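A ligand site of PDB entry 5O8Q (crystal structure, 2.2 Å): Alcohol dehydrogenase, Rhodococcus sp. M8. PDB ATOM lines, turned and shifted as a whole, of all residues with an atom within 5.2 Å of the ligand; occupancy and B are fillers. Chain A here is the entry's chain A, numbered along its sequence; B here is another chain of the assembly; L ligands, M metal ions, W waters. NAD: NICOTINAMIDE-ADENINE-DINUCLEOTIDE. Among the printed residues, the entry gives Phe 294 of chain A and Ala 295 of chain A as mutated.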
ATOM      1  N   CYS A  38     -26.643 -12.992 -18.048  1.00  0.00           N
ATOM      2  CA  CYS A  38     -25.974 -14.105 -18.731  1.00  0.00           C
ATOM      3  C   CYS A  38     -26.973 -15.107 -19.318  1.00  0.00           C
ATOM      4  O   CYS A  38     -28.165 -15.088 -19.013  1.00  0.00           O
ATOM      5  CB  CYS A  38     -24.987 -14.834 -17.812  1.00  0.00           C
ATOM      6  SG  CYS A  38     -23.897 -16.025 -18.691  1.00  0.00           S
ATOM      7  N   HIS A  39     -26.442 -15.984 -20.166  1.00  0.00           N
ATOM      8  CA  HIS A  39     -27.244 -17.055 -20.764  1.00  0.00           C
ATOM      9  C   HIS A  39     -27.779 -18.113 -19.766  1.00  0.00           C
ATOM     10  O   HIS A  39     -28.697 -18.856 -20.114  1.00  0.00           O
ATOM     11  CB  HIS A  39     -26.453 -17.741 -21.865  1.00  0.00           C
ATOM     12  CG  HIS A  39     -26.242 -16.869 -23.069  1.00  0.00           C
ATOM     13  ND1 HIS A  39     -26.962 -17.021 -24.232  1.00  0.00           N
ATOM     14  CD2 HIS A  39     -25.374 -15.862 -23.292  1.00  0.00           C
ATOM     15  CE1 HIS A  39     -26.553 -16.140 -25.122  1.00  0.00           C
ATOM     16  NE2 HIS A  39     -25.576 -15.428 -24.576  1.00  0.00           N
ATOM     17  N   SER A  40     -27.252 -18.183 -18.566  1.00  0.00           N
ATOM     18  CA  SER A  40     -27.806 -19.063 -17.528  1.00  0.00           C
ATOM     19  C   SER A  40     -29.285 -18.696 -17.215  1.00  0.00           C
ATOM     20  O   SER A  40     -30.119 -19.588 -17.008  1.00  0.00           O
ATOM     21  CB  SER A  40     -27.008 -19.047 -16.204  1.00  0.00           C
ATOM     22  OG  SER A  40     -25.603 -18.725 -16.124  1.00  0.00           O
ATOM     23  N   ASP A 153     -18.881 -13.915 -13.038  1.00  0.00           N
ATOM     24  CA  ASP A 153     -19.047 -15.087 -13.925  1.00  0.00           C
ATOM     25  C   ASP A 153     -18.316 -14.949 -15.266  1.00  0.00           C
ATOM     26  O   ASP A 153     -17.561 -15.841 -15.637  1.00  0.00           O
ATOM     27  CB  ASP A 153     -20.530 -15.408 -14.119  1.00  0.00           C
ATOM     28  CG  ASP A 153     -20.805 -16.875 -14.463  1.00  0.00           C
ATOM     29  OD1 ASP A 153     -20.006 -17.793 -14.138  1.00  0.00           O
ATOM     30  OD2 ASP A 153     -21.862 -17.129 -15.061  1.00  0.00           O
ATOM     31  N   THR A 157     -15.410 -17.656 -14.617  1.00  0.00           N
ATOM     32  CA  THR A 157     -15.464 -18.868 -15.407  1.00  0.00           C
ATOM     33  C   THR A 157     -14.249 -19.028 -16.338  1.00  0.00           C
ATOM     34  O   THR A 157     -13.594 -20.074 -16.299  1.00  0.00           O
ATOM     35  CB  THR A 157     -16.805 -18.967 -16.163  1.00  0.00           C
ATOM     36  OG1 THR A 157     -17.864 -19.098 -15.197  1.00  0.00           O
ATOM     37  CG2 THR A 157     -16.850 -20.167 -17.090  1.00  0.00           C
ATOM     38  N   ILE A 178     -12.137 -19.071 -28.559  1.00  0.00           N
ATOM     39  CA  ILE A 178     -13.237 -19.093 -29.526  1.00  0.00           C
ATOM     40  C   ILE A 178     -14.471 -18.435 -28.885  1.00  0.00           C
ATOM     41  O   ILE A 178     -14.969 -18.900 -27.865  1.00  0.00           O
ATOM     42  CB  ILE A 178     -13.582 -20.499 -30.018  1.00  0.00           C
ATOM     43  CG1 ILE A 178     -12.305 -21.234 -30.483  1.00  0.00           C
ATOM     44  CG2 ILE A 178     -14.616 -20.437 -31.144  1.00  0.00           C
ATOM     45  CD1 ILE A 178     -12.530 -22.627 -31.006  1.00  0.00           C
ATOM     46  N   GLY A 179     -14.949 -17.350 -29.508  1.00  0.00           N
ATOM     47  CA  GLY A 179     -16.097 -16.608 -29.021  1.00  0.00           C
ATOM     48  C   GLY A 179     -15.657 -15.416 -28.218  1.00  0.00           C
ATOM     49  O   GLY A 179     -15.175 -15.594 -27.093  1.00  0.00           O
ATOM     50  N   VAL A 180     -15.810 -14.220 -28.780  1.00  0.00           N
ATOM     51  CA  VAL A 180     -15.377 -12.977 -28.130  1.00  0.00           C
ATOM     52  C   VAL A 180     -16.603 -12.167 -27.666  1.00  0.00           C
ATOM     53  O   VAL A 180     -16.898 -11.105 -28.187  1.00  0.00           O
ATOM     54  CB  VAL A 180     -14.447 -12.154 -29.063  1.00  0.00           C
ATOM     55  CG1 VAL A 180     -13.822 -10.978 -28.306  1.00  0.00           C
ATOM     56  CG2 VAL A 180     -13.329 -13.048 -29.594  1.00  0.00           C
ATOM     57  N   GLY A 181     -17.291 -12.702 -26.667  1.00  0.00           N
ATOM     58  CA  GLY A 181     -18.455 -12.040 -26.063  1.00  0.00           C
ATOM     59  C   GLY A 181     -18.158 -11.703 -24.603  1.00  0.00           C
ATOM     60  O   GLY A 181     -17.032 -11.325 -24.271  1.00  0.00           O
ATOM     61  N   GLY A 182     -19.172 -11.849 -23.750  1.00  0.00           N
ATOM     62  CA  GLY A 182     -18.972 -11.584 -22.315  1.00  0.00           C
ATOM     63  C   GLY A 182     -17.791 -12.298 -21.722  1.00  0.00           C
ATOM     64  O   GLY A 182     -16.885 -11.661 -21.180  1.00  0.00           O
ATOM     65  N   LEU A 183     -17.794 -13.625 -21.808  1.00  0.00           N
ATOM     66  CA  LEU A 183     -16.691 -14.451 -21.283  1.00  0.00           C
ATOM     67  C   LEU A 183     -15.398 -14.298 -22.103  1.00  0.00           C
ATOM     68  O   LEU A 183     -14.335 -14.061 -21.530  1.00  0.00           O
ATOM     69  CB  LEU A 183     -17.096 -15.928 -21.218  1.00  0.00           C
ATOM     70  CG  LEU A 183     -17.802 -16.369 -19.947  1.00  0.00           C
ATOM     71  CD1 LEU A 183     -19.176 -15.751 -19.839  1.00  0.00           C
ATOM     72  CD2 LEU A 183     -17.924 -17.872 -19.865  1.00  0.00           C
ATOM     73  N   GLY A 184     -15.480 -14.426 -23.419  1.00  0.00           N
ATOM     74  CA  GLY A 184     -14.286 -14.457 -24.255  1.00  0.00           C
ATOM     75  C   GLY A 184     -13.391 -13.232 -24.224  1.00  0.00           C
ATOM     76  O   GLY A 184     -12.169 -13.355 -24.242  1.00  0.00           O
ATOM     77  N   VAL A 202     -11.010 -16.025 -32.089  1.00  0.00           N
ATOM     78  CA  VAL A 202     -11.825 -16.539 -33.192  1.00  0.00           C
ATOM     79  C   VAL A 202     -13.277 -16.152 -32.957  1.00  0.00           C
ATOM     80  O   VAL A 202     -13.785 -16.326 -31.844  1.00  0.00           O
ATOM     81  CB  VAL A 202     -11.736 -18.081 -33.326  1.00  0.00           C
ATOM     82  CG1 VAL A 202     -12.546 -18.582 -34.543  1.00  0.00           C
ATOM     83  CG2 VAL A 202     -10.293 -18.524 -33.421  1.00  0.00           C
ATOM     84  N   ASP A 203     -13.943 -15.612 -33.987  1.00  0.00           N
ATOM     85  CA  ASP A 203     -15.363 -15.274 -33.906  1.00  0.00           C
ATOM     86  C   ASP A 203     -15.965 -15.266 -35.324  1.00  0.00           C
ATOM     87  O   ASP A 203     -15.218 -15.225 -36.313  1.00  0.00           O
ATOM     88  CB  ASP A 203     -15.564 -13.922 -33.210  1.00  0.00           C
ATOM     89  CG  ASP A 203     -16.939 -13.783 -32.529  1.00  0.00           C
ATOM     90  OD1 ASP A 203     -17.973 -13.718 -33.236  1.00  0.00           O
ATOM     91  OD2 ASP A 203     -16.967 -13.699 -31.270  1.00  0.00           O
ATOM     92  N   LEU A 204     -17.301 -15.309 -35.394  1.00  0.00           N
ATOM     93  CA  LEU A 204     -18.026 -15.180 -36.674  1.00  0.00           C
ATOM     94  C   LEU A 204     -18.121 -13.759 -37.219  1.00  0.00           C
ATOM     95  O   LEU A 204     -18.259 -13.566 -38.422  1.00  0.00           O
ATOM     96  CB  LEU A 204     -19.474 -15.678 -36.510  1.00  0.00           C
ATOM     97  CG  LEU A 204     -19.762 -17.163 -36.511  1.00  0.00           C
ATOM     98  CD1 LEU A 204     -21.231 -17.363 -36.105  1.00  0.00           C
ATOM     99  CD2 LEU A 204     -19.518 -17.739 -37.920  1.00  0.00           C
ATOM    100  N   ASP A 205     -18.059 -12.790 -36.323  1.00  0.00           N
ATOM    101  CA  ASP A 205     -18.430 -11.400 -36.586  1.00  0.00           C
ATOM    102  C   ASP A 205     -17.172 -10.547 -36.628  1.00  0.00           C
ATOM    103  O   ASP A 205     -16.378 -10.583 -35.668  1.00  0.00           O
ATOM    104  CB  ASP A 205     -19.348 -10.975 -35.421  1.00  0.00           C
ATOM    105  CG  ASP A 205     -20.031  -9.645 -35.617  1.00  0.00           C
ATOM    106  OD1 ASP A 205     -19.700  -8.885 -36.570  1.00  0.00           O
ATOM    107  OD2 ASP A 205     -20.919  -9.359 -34.778  1.00  0.00           O
ATOM    108  N   ARG A 208     -16.592  -8.338 -33.590  1.00  0.00           N
ATOM    109  CA  ARG A 208     -16.035  -9.045 -32.431  1.00  0.00           C
ATOM    110  C   ARG A 208     -14.529  -9.318 -32.582  1.00  0.00           C
ATOM    111  O   ARG A 208     -13.824  -9.336 -31.591  1.00  0.00           O
ATOM    112  CB  ARG A 208     -16.801 -10.341 -32.162  1.00  0.00           C
ATOM    113  CG  ARG A 208     -18.290 -10.158 -31.903  1.00  0.00           C
ATOM    114  CD  ARG A 208     -18.587  -9.277 -30.720  1.00  0.00           C
ATOM    115  NE  ARG A 208     -20.024  -9.098 -30.556  1.00  0.00           N
ATOM    116  CZ  ARG A 208     -20.777  -9.545 -29.543  1.00  0.00           C
ATOM    117  NH1 ARG A 208     -20.254 -10.208 -28.514  1.00  0.00           N
ATOM    118  NH2 ARG A 208     -22.070  -9.295 -29.523  1.00  0.00           N
ATOM    119  N   SER A 223     -14.103 -17.437 -37.784  1.00  0.00           N
ATOM    120  CA  SER A 223     -14.513 -18.821 -37.503  1.00  0.00           C
ATOM    121  C   SER A 223     -14.992 -19.543 -38.786  1.00  0.00           C
ATOM    122  O   SER A 223     -15.090 -18.940 -39.841  1.00  0.00           O
ATOM    123  CB  SER A 223     -15.619 -18.816 -36.417  1.00  0.00           C
ATOM    124  OG  SER A 223     -16.855 -18.165 -36.754  1.00  0.00           O
ATOM    125  N   PHE A 246     -15.520 -20.801 -25.808  1.00  0.00           N
ATOM    126  CA  PHE A 246     -16.638 -20.161 -25.132  1.00  0.00           C
ATOM    127  C   PHE A 246     -17.920 -20.151 -25.966  1.00  0.00           C
ATOM    128  O   PHE A 246     -18.893 -19.505 -25.585  1.00  0.00           O
ATOM    129  CB  PHE A 246     -16.249 -18.729 -24.705  1.00  0.00           C
ATOM    130  CG  PHE A 246     -15.058 -18.685 -23.779  1.00  0.00           C
ATOM    131  CD1 PHE A 246     -15.163 -19.065 -22.452  1.00  0.00           C
ATOM    132  CD2 PHE A 246     -13.822 -18.265 -24.240  1.00  0.00           C
ATOM    133  CE1 PHE A 246     -14.055 -19.041 -21.616  1.00  0.00           C
ATOM    134  CE2 PHE A 246     -12.716 -18.221 -23.393  1.00  0.00           C
ATOM    135  CZ  PHE A 246     -12.846 -18.612 -22.088  1.00  0.00           C
ATOM    136  N   VAL A 247     -17.941 -20.857 -27.100  1.00  0.00           N
ATOM    137  CA  VAL A 247     -19.185 -21.062 -27.876  1.00  0.00           C
ATOM    138  C   VAL A 247     -19.722 -22.464 -27.576  1.00  0.00           C
ATOM    139  O   VAL A 247     -20.832 -22.624 -27.082  1.00  0.00           O
ATOM    140  CB  VAL A 247     -18.940 -20.888 -29.381  1.00  0.00           C
ATOM    141  CG1 VAL A 247     -20.220 -21.054 -30.177  1.00  0.00           C
ATOM    142  CG2 VAL A 247     -18.351 -19.527 -29.681  1.00  0.00           C
ATOM    143  N   ALA A 249     -20.412 -24.896 -29.733  1.00  0.00           N
ATOM    144  CA  ALA A 249     -21.204 -25.520 -30.798  1.00  0.00           C
ATOM    145  C   ALA A 249     -20.375 -26.658 -31.371  1.00  0.00           C
ATOM    146  O   ALA A 249     -19.150 -26.709 -31.170  1.00  0.00           O
ATOM    147  CB  ALA A 249     -21.552 -24.515 -31.882  1.00  0.00           C
ATOM    148  N   SER A 251     -19.488 -27.275 -34.423  1.00  0.00           N
ATOM    149  CA  SER A 251     -18.493 -26.751 -35.372  1.00  0.00           C
ATOM    150  C   SER A 251     -17.260 -26.117 -34.685  1.00  0.00           C
ATOM    151  O   SER A 251     -16.155 -26.229 -35.203  1.00  0.00           O
ATOM    152  CB  SER A 251     -19.136 -25.783 -36.365  1.00  0.00           C
ATOM    153  OG  SER A 251     -19.566 -24.617 -35.699  1.00  0.00           O
ATOM    154  N   THR A 252     -17.437 -25.460 -33.539  1.00  0.00           N
ATOM    155  CA  THR A 252     -16.294 -24.862 -32.814  1.00  0.00           C
ATOM    156  C   THR A 252     -15.465 -25.907 -32.067  1.00  0.00           C
ATOM    157  O   THR A 252     -14.239 -25.786 -32.009  1.00  0.00           O
ATOM    158  CB  THR A 252     -16.717 -23.744 -31.852  1.00  0.00           C
ATOM    159  OG1 THR A 252     -17.549 -24.255 -30.805  1.00  0.00           O
ATOM    160  CG2 THR A 252     -17.435 -22.632 -32.640  1.00  0.00           C
ATOM    161  N   VAL A 269     -16.255 -24.574 -22.626  1.00  0.00           N
ATOM    162  CA  VAL A 269     -16.901 -23.723 -21.631  1.00  0.00           C
ATOM    163  C   VAL A 269     -18.291 -23.328 -22.058  1.00  0.00           C
ATOM    164  O   VAL A 269     -19.211 -23.332 -21.261  1.00  0.00           O
ATOM    165  CB  VAL A 269     -16.069 -22.451 -21.356  1.00  0.00           C
ATOM    166  CG1 VAL A 269     -16.706 -21.610 -20.257  1.00  0.00           C
ATOM    167  CG2 VAL A 269     -14.647 -22.833 -20.978  1.00  0.00           C
ATOM    168  N   GLY A 270     -18.446 -22.970 -23.321  1.00  0.00           N
ATOM    169  CA  GLY A 270     -19.768 -22.672 -23.876  1.00  0.00           C
ATOM    170  C   GLY A 270     -20.695 -23.877 -23.902  1.00  0.00           C
ATOM    171  O   GLY A 270     -20.253 -25.011 -24.059  1.00  0.00           O
ATOM    172  N   ILE A 271     -22.002 -23.596 -23.773  1.00  0.00           N
ATOM    173  CA  ILE A 271     -23.036 -24.607 -23.632  1.00  0.00           C
ATOM    174  C   ILE A 271     -23.995 -24.582 -24.825  1.00  0.00           C
ATOM    175  O   ILE A 271     -24.759 -23.638 -24.979  1.00  0.00           O
ATOM    176  CB  ILE A 271     -23.834 -24.387 -22.313  1.00  0.00           C
ATOM    177  CG1 ILE A 271     -22.888 -24.415 -21.109  1.00  0.00           C
ATOM    178  CG2 ILE A 271     -24.948 -25.428 -22.182  1.00  0.00           C
ATOM    179  CD1 ILE A 271     -23.538 -23.934 -19.812  1.00  0.00           C
ATOM    180  N   PRO A 293     -15.496 -27.285 -17.842  1.00  0.00           N
ATOM    181  CA  PRO A 293     -15.411 -26.737 -16.488  1.00  0.00           C
ATOM    182  C   PRO A 293     -16.696 -25.971 -16.129  1.00  0.00           C
ATOM    183  O   PRO A 293     -17.497 -25.641 -17.010  1.00  0.00           O
ATOM    184  CB  PRO A 293     -14.207 -25.814 -16.561  1.00  0.00           C
ATOM    185  CG  PRO A 293     -14.216 -25.309 -17.979  1.00  0.00           C
ATOM    186  CD  PRO A 293     -14.913 -26.365 -18.826  1.00  0.00           C
ATOM    187  N   PHE A 294     -16.902 -25.734 -14.848  1.00  0.00           N
ATOM    188  CA  PHE A 294     -18.084 -25.025 -14.348  1.00  0.00           C
ATOM    189  C   PHE A 294     -17.666 -23.961 -13.350  1.00  0.00           C
ATOM    190  O   PHE A 294     -17.037 -24.258 -12.335  1.00  0.00           O
ATOM    191  CB  PHE A 294     -19.057 -25.995 -13.691  1.00  0.00           C
ATOM    192  CG  PHE A 294     -20.292 -25.317 -13.135  1.00  0.00           C
ATOM    193  CD1 PHE A 294     -21.194 -24.682 -13.977  1.00  0.00           C
ATOM    194  CD2 PHE A 294     -20.541 -25.309 -11.757  1.00  0.00           C
ATOM    195  CE1 PHE A 294     -22.334 -24.065 -13.483  1.00  0.00           C
ATOM    196  CE2 PHE A 294     -21.685 -24.681 -11.246  1.00  0.00           C
ATOM    197  CZ  PHE A 294     -22.579 -24.053 -12.118  1.00  0.00           C
ATOM    198  N   ALA A 295     -18.004 -22.715 -13.672  1.00  0.00           N
ATOM    199  CA  ALA A 295     -17.845 -21.580 -12.751  1.00  0.00           C
ATOM    200  C   ALA A 295     -16.403 -21.479 -12.226  1.00  0.00           C
ATOM    201  O   ALA A 295     -15.491 -21.538 -13.033  1.00  0.00           O
ATOM    202  CB  ALA A 295     -18.905 -21.637 -11.640  1.00  0.00           C
ATOM    203  N   LEU A 332     -30.007  -9.779 -25.493  1.00  0.00           N
ATOM    204  CA  LEU A 332     -29.077 -10.895 -25.256  1.00  0.00           C
ATOM    205  C   LEU A 332     -29.389 -12.113 -26.134  1.00  0.00           C
ATOM    206  O   LEU A 332     -28.469 -12.737 -26.649  1.00  0.00           O
ATOM    207  CB  LEU A 332     -29.051 -11.283 -23.776  1.00  0.00           C
ATOM    208  CG  LEU A 332     -28.008 -12.313 -23.352  1.00  0.00           C
ATOM    209  CD1 LEU A 332     -26.581 -11.888 -23.702  1.00  0.00           C
ATOM    210  CD2 LEU A 332     -28.119 -12.603 -21.854  1.00  0.00           C
ATOM    211  N   GLY A 339     -20.161  -7.121 -25.445  1.00  0.00           N
ATOM    212  CA  GLY A 339     -19.608  -7.415 -24.124  1.00  0.00           C
ATOM    213  C   GLY A 339     -20.719  -7.908 -23.208  1.00  0.00           C
ATOM    214  O   GLY A 339     -21.553  -8.706 -23.611  1.00  0.00           O
ATOM    215  N   ARG A 340     -20.738  -7.378 -21.985  1.00  0.00           N
ATOM    216  CA  ARG A 340     -21.634  -7.851 -20.927  1.00  0.00           C
ATOM    217  C   ARG A 340     -22.747  -6.838 -20.648  1.00  0.00           C
ATOM    218  O   ARG A 340     -22.460  -5.676 -20.363  1.00  0.00           O
ATOM    219  CB  ARG A 340     -20.829  -8.022 -19.640  1.00  0.00           C
ATOM    220  CG  ARG A 340     -21.013  -9.305 -18.846  1.00  0.00           C
ATOM    221  CD  ARG A 340     -22.372  -9.955 -18.760  1.00  0.00           C
ATOM    222  NE  ARG A 340     -22.110 -11.351 -18.373  1.00  0.00           N
ATOM    223  CZ  ARG A 340     -21.939 -12.373 -19.209  1.00  0.00           C
ATOM    224  NH1 ARG A 340     -22.035 -12.243 -20.509  1.00  0.00           N
ATOM    225  NH2 ARG A 340     -21.699 -13.563 -18.717  1.00  0.00           N
ATOM    226  N   PHE B 281     -21.605 -30.951 -22.237  1.00  0.00           N
ATOM    227  CA  PHE B 281     -22.459 -30.694 -21.085  1.00  0.00           C
ATOM    228  C   PHE B 281     -23.636 -31.678 -21.087  1.00  0.00           C
ATOM    229  O   PHE B 281     -24.162 -32.010 -22.156  1.00  0.00           O
ATOM    230  CB  PHE B 281     -22.912 -29.240 -21.022  1.00  0.00           C
ATOM    231  CG  PHE B 281     -21.802 -28.294 -20.664  1.00  0.00           C
ATOM    232  CD1 PHE B 281     -21.526 -27.999 -19.339  1.00  0.00           C
ATOM    233  CD2 PHE B 281     -21.003 -27.719 -21.650  1.00  0.00           C
ATOM    234  CE1 PHE B 281     -20.484 -27.147 -18.996  1.00  0.00           C
ATOM    235  CE2 PHE B 281     -19.968 -26.864 -21.324  1.00  0.00           C
ATOM    236  CZ  PHE B 281     -19.694 -26.578 -19.993  1.00  0.00           C
HETATM  237  PA  NAD L   1     -22.273 -13.904 -25.406  1.00  0.00           P
HETATM  238  O1A NAD L   1     -23.593 -14.000 -26.112  1.00  0.00           O
HETATM  239  O2A NAD L   1     -21.861 -12.653 -24.707  1.00  0.00           O
HETATM  240  O5B NAD L   1     -21.107 -14.206 -26.487  1.00  0.00           O
HETATM  241  C5B NAD L   1     -21.295 -14.924 -27.698  1.00  0.00           C
HETATM  242  C4B NAD L   1     -20.070 -14.695 -28.581  1.00  0.00           C
HETATM  243  O4B NAD L   1     -19.826 -15.886 -29.331  1.00  0.00           O
HETATM  244  C3B NAD L   1     -20.257 -13.589 -29.597  1.00  0.00           C
HETATM  245  O3B NAD L   1     -19.021 -12.894 -29.773  1.00  0.00           O
HETATM  246  C2B NAD L   1     -20.692 -14.324 -30.850  1.00  0.00           C
HETATM  247  O2B NAD L   1     -20.406 -13.633 -32.068  1.00  0.00           O
HETATM  248  C1B NAD L   1     -19.870 -15.599 -30.729  1.00  0.00           C
HETATM  249  N9A NAD L   1     -20.375 -16.780 -31.469  1.00  0.00           N
HETATM  250  C8A NAD L   1     -21.631 -17.288 -31.437  1.00  0.00           C
HETATM  251  N7A NAD L   1     -21.696 -18.392 -32.225  1.00  0.00           N
HETATM  252  C5A NAD L   1     -20.484 -18.602 -32.766  1.00  0.00           C
HETATM  253  C6A NAD L   1     -19.858 -19.598 -33.675  1.00  0.00           C
HETATM  254  N6A NAD L   1     -20.599 -20.607 -34.178  1.00  0.00           N
HETATM  255  N1A NAD L   1     -18.551 -19.463 -33.991  1.00  0.00           N
HETATM  256  C2A NAD L   1     -17.799 -18.467 -33.490  1.00  0.00           C
HETATM  257  N3A NAD L   1     -18.307 -17.542 -32.654  1.00  0.00           N
HETATM  258  C4A NAD L   1     -19.610 -17.549 -32.262  1.00  0.00           C
HETATM  259  O3  NAD L   1     -22.175 -15.197 -24.449  1.00  0.00           O
HETATM  260  PN  NAD L   1     -21.386 -15.246 -23.038  1.00  0.00           P
HETATM  261  O1N NAD L   1     -22.274 -14.626 -22.012  1.00  0.00           O
HETATM  262  O2N NAD L   1     -19.962 -14.785 -23.232  1.00  0.00           O
HETATM  263  O5D NAD L   1     -21.392 -16.850 -22.784  1.00  0.00           O
HETATM  264  C5D NAD L   1     -20.804 -17.747 -23.752  1.00  0.00           C
HETATM  265  C4D NAD L   1     -21.193 -19.194 -23.475  1.00  0.00           C
HETATM  266  O4D NAD L   1     -20.693 -19.611 -22.197  1.00  0.00           O
HETATM  267  C3D NAD L   1     -22.688 -19.449 -23.424  1.00  0.00           C
HETATM  268  O3D NAD L   1     -22.917 -20.704 -24.070  1.00  0.00           O
HETATM  269  C2D NAD L   1     -23.009 -19.548 -21.947  1.00  0.00           C
HETATM  270  O2D NAD L   1     -24.152 -20.354 -21.682  1.00  0.00           O
HETATM  271  C1D NAD L   1     -21.739 -20.217 -21.436  1.00  0.00           C
HETATM  272  N1N NAD L   1     -21.381 -20.078 -20.020  1.00  0.00           N
HETATM  273  C2N NAD L   1     -20.838 -21.148 -19.416  1.00  0.00           C
HETATM  274  C3N NAD L   1     -20.431 -21.124 -18.085  1.00  0.00           C
HETATM  275  C7N NAD L   1     -19.807 -22.325 -17.430  1.00  0.00           C
HETATM  276  O7N NAD L   1     -19.693 -22.341 -16.210  1.00  0.00           O
HETATM  277  N7N NAD L   1     -19.328 -23.356 -18.134  1.00  0.00           N
HETATM  278  C4N NAD L   1     -20.584 -19.933 -17.375  1.00  0.00           C
HETATM  279  C5N NAD L   1     -21.129 -18.817 -18.019  1.00  0.00           C
HETATM  280  C6N NAD L   1     -21.515 -18.904 -19.354  1.00  0.00           C
HETATM  281 ZN    ZN M   1     -23.309 -17.217 -16.314  1.00  0.00          ZN
HETATM  282  O   HOH W   1     -21.539 -10.267 -26.038  1.00  0.00           O
HETATM  283  O   HOH W   2     -18.068 -22.127 -36.085  1.00  0.00           O
HETATM  284  O   HOH W   3     -22.591 -20.711 -26.749  1.00  0.00           O
HETATM  285  O   HOH W   4     -25.539 -21.220 -23.778  1.00  0.00           O
HETATM  286  O   HOH W   5     -17.893 -15.164 -24.895  1.00  0.00           O
HETATM  287  O   HOH W   6     -18.717 -17.073 -26.713  1.00  0.00           O
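Water W4 bridges O2D of the ligand (2.7 Å) and O of Ile 271 (2.8 Å).
Water W3 bridges O of Val 247 (2.6 Å) and O3D of the ligand (2.7 Å).
Water W1 lies within hydrogen-bond range of O2A of the ligand (2.8 Å), NH1 of Arg 208 (2.8 Å) and O of Gly 339 (2.9 Å).
Water W6 bridges O of Phe 246 and O4B of the ligand.
Water W2 bridges the side-chain hydroxyl of Ser 251 (2.9 Å) and a nitrogen (N1A) of the ligand (3.4 Å).
An oxygen (O3B) of the ligand is in hydrogen-bond range of the side-chain carboxylate (OD2) of Asp 203 (2.7 Å).
The guanidinium group of Arg 340 lies within salt-bridge range of an oxygen (O1N) of the ligand (2.8 Å).
N of Leu 183 lies within hydrogen-bond range of O2N of the ligand (2.8 Å).
O1A of the ligand sits at hydrogen-bond distance from NE2 of His 39 (2.9 Å).
O2A of the ligand is in hydrogen-bond range of N of Gly 182 (3.0 Å).
The backbone NH (N) of Ile 271 sits at hydrogen-bond distance from an oxygen (O3D) of the ligand (3.0 Å).
The backbone NH (N) of Ala 295 lies within hydrogen-bond range of an oxygen (O7N) of the ligand (3.1 Å).
N7N of the ligand lies within hydrogen-bond range of O of Val 269, 3.1 Å away.
O of Pro 293 lies within hydrogen-bond range of N7N of the ligand (3.1 Å).
O of Val 180 sits at hydrogen-bond distance from O3B of the ligand (3.2 Å).
An oxygen (O3B) of the ligand is in hydrogen-bond range of the guanidinium group (NH1) of Arg 208, at 3.2 Å.
The side-chain hydroxyl (OG) of Ser 223 lies close to a nitrogen (N1A) of the ligand (3.5 Å).
SG of Cys 38 touches C6N of the ligand (3.8 Å).
Asp 153 touches the ligand (OD2 to C5N, 3.5 Å).
OG1 of Thr 157 touches C4N of the ligand, 3.6 Å away.
Gly 179 touches the ligand.
Gly 181 touches the ligand (CA to O5B, 3.5 Å).
CD1 of Leu 204 touches C6A of the ligand, at 3.6 Å.
Phe 246 touches the ligand (O to C4D, 3.1 Å).
Val 247 touches the ligand (CG2 to C4A, 3.5 Å).
Thr 252 touches the ligand.
Gly 270 touches the ligand.
Phe 294 touches the ligand.
Phe 281 of chain B touches the ligand (CZ to N7N, 3.7 Å).
The nearest printed residue that does not touch the ligand is Gly 339 (4.1 Å).
The backbone NH of Val 180 is in hydrogen-bond range of the side-chain carboxylate of Asp 203, 2.8 Å away.
N of Ser 223 is in hydrogen-bond range of O of Asp 203.
NH2 of Arg 340 sits close to SG of Cys 38.
The backbone NH (N) of Phe 246 is in hydrogen-bond range of the backbone carbonyl oxygen (O) of Ile 178, at 2.9 Å.
The guanidinium group (NH1) of Arg 208 sits at hydrogen-bond distance from the backbone carbonyl oxygen (O) of Val 180, 3.5 Å away.
N of Leu 204 lies close to OG of Ser 223, 3.2 Å away.
The side-chain carboxylate (OD1) of Asp 153 sits at hydrogen-bond distance from the side-chain hydroxyl (OG1) of Thr 157, 2.7 Å away.
The side-chain hydroxyl (OG1) of Thr 252 sits at hydrogen-bond distance from the backbone carbonyl oxygen (O) of Ala 249 (3.0 Å).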
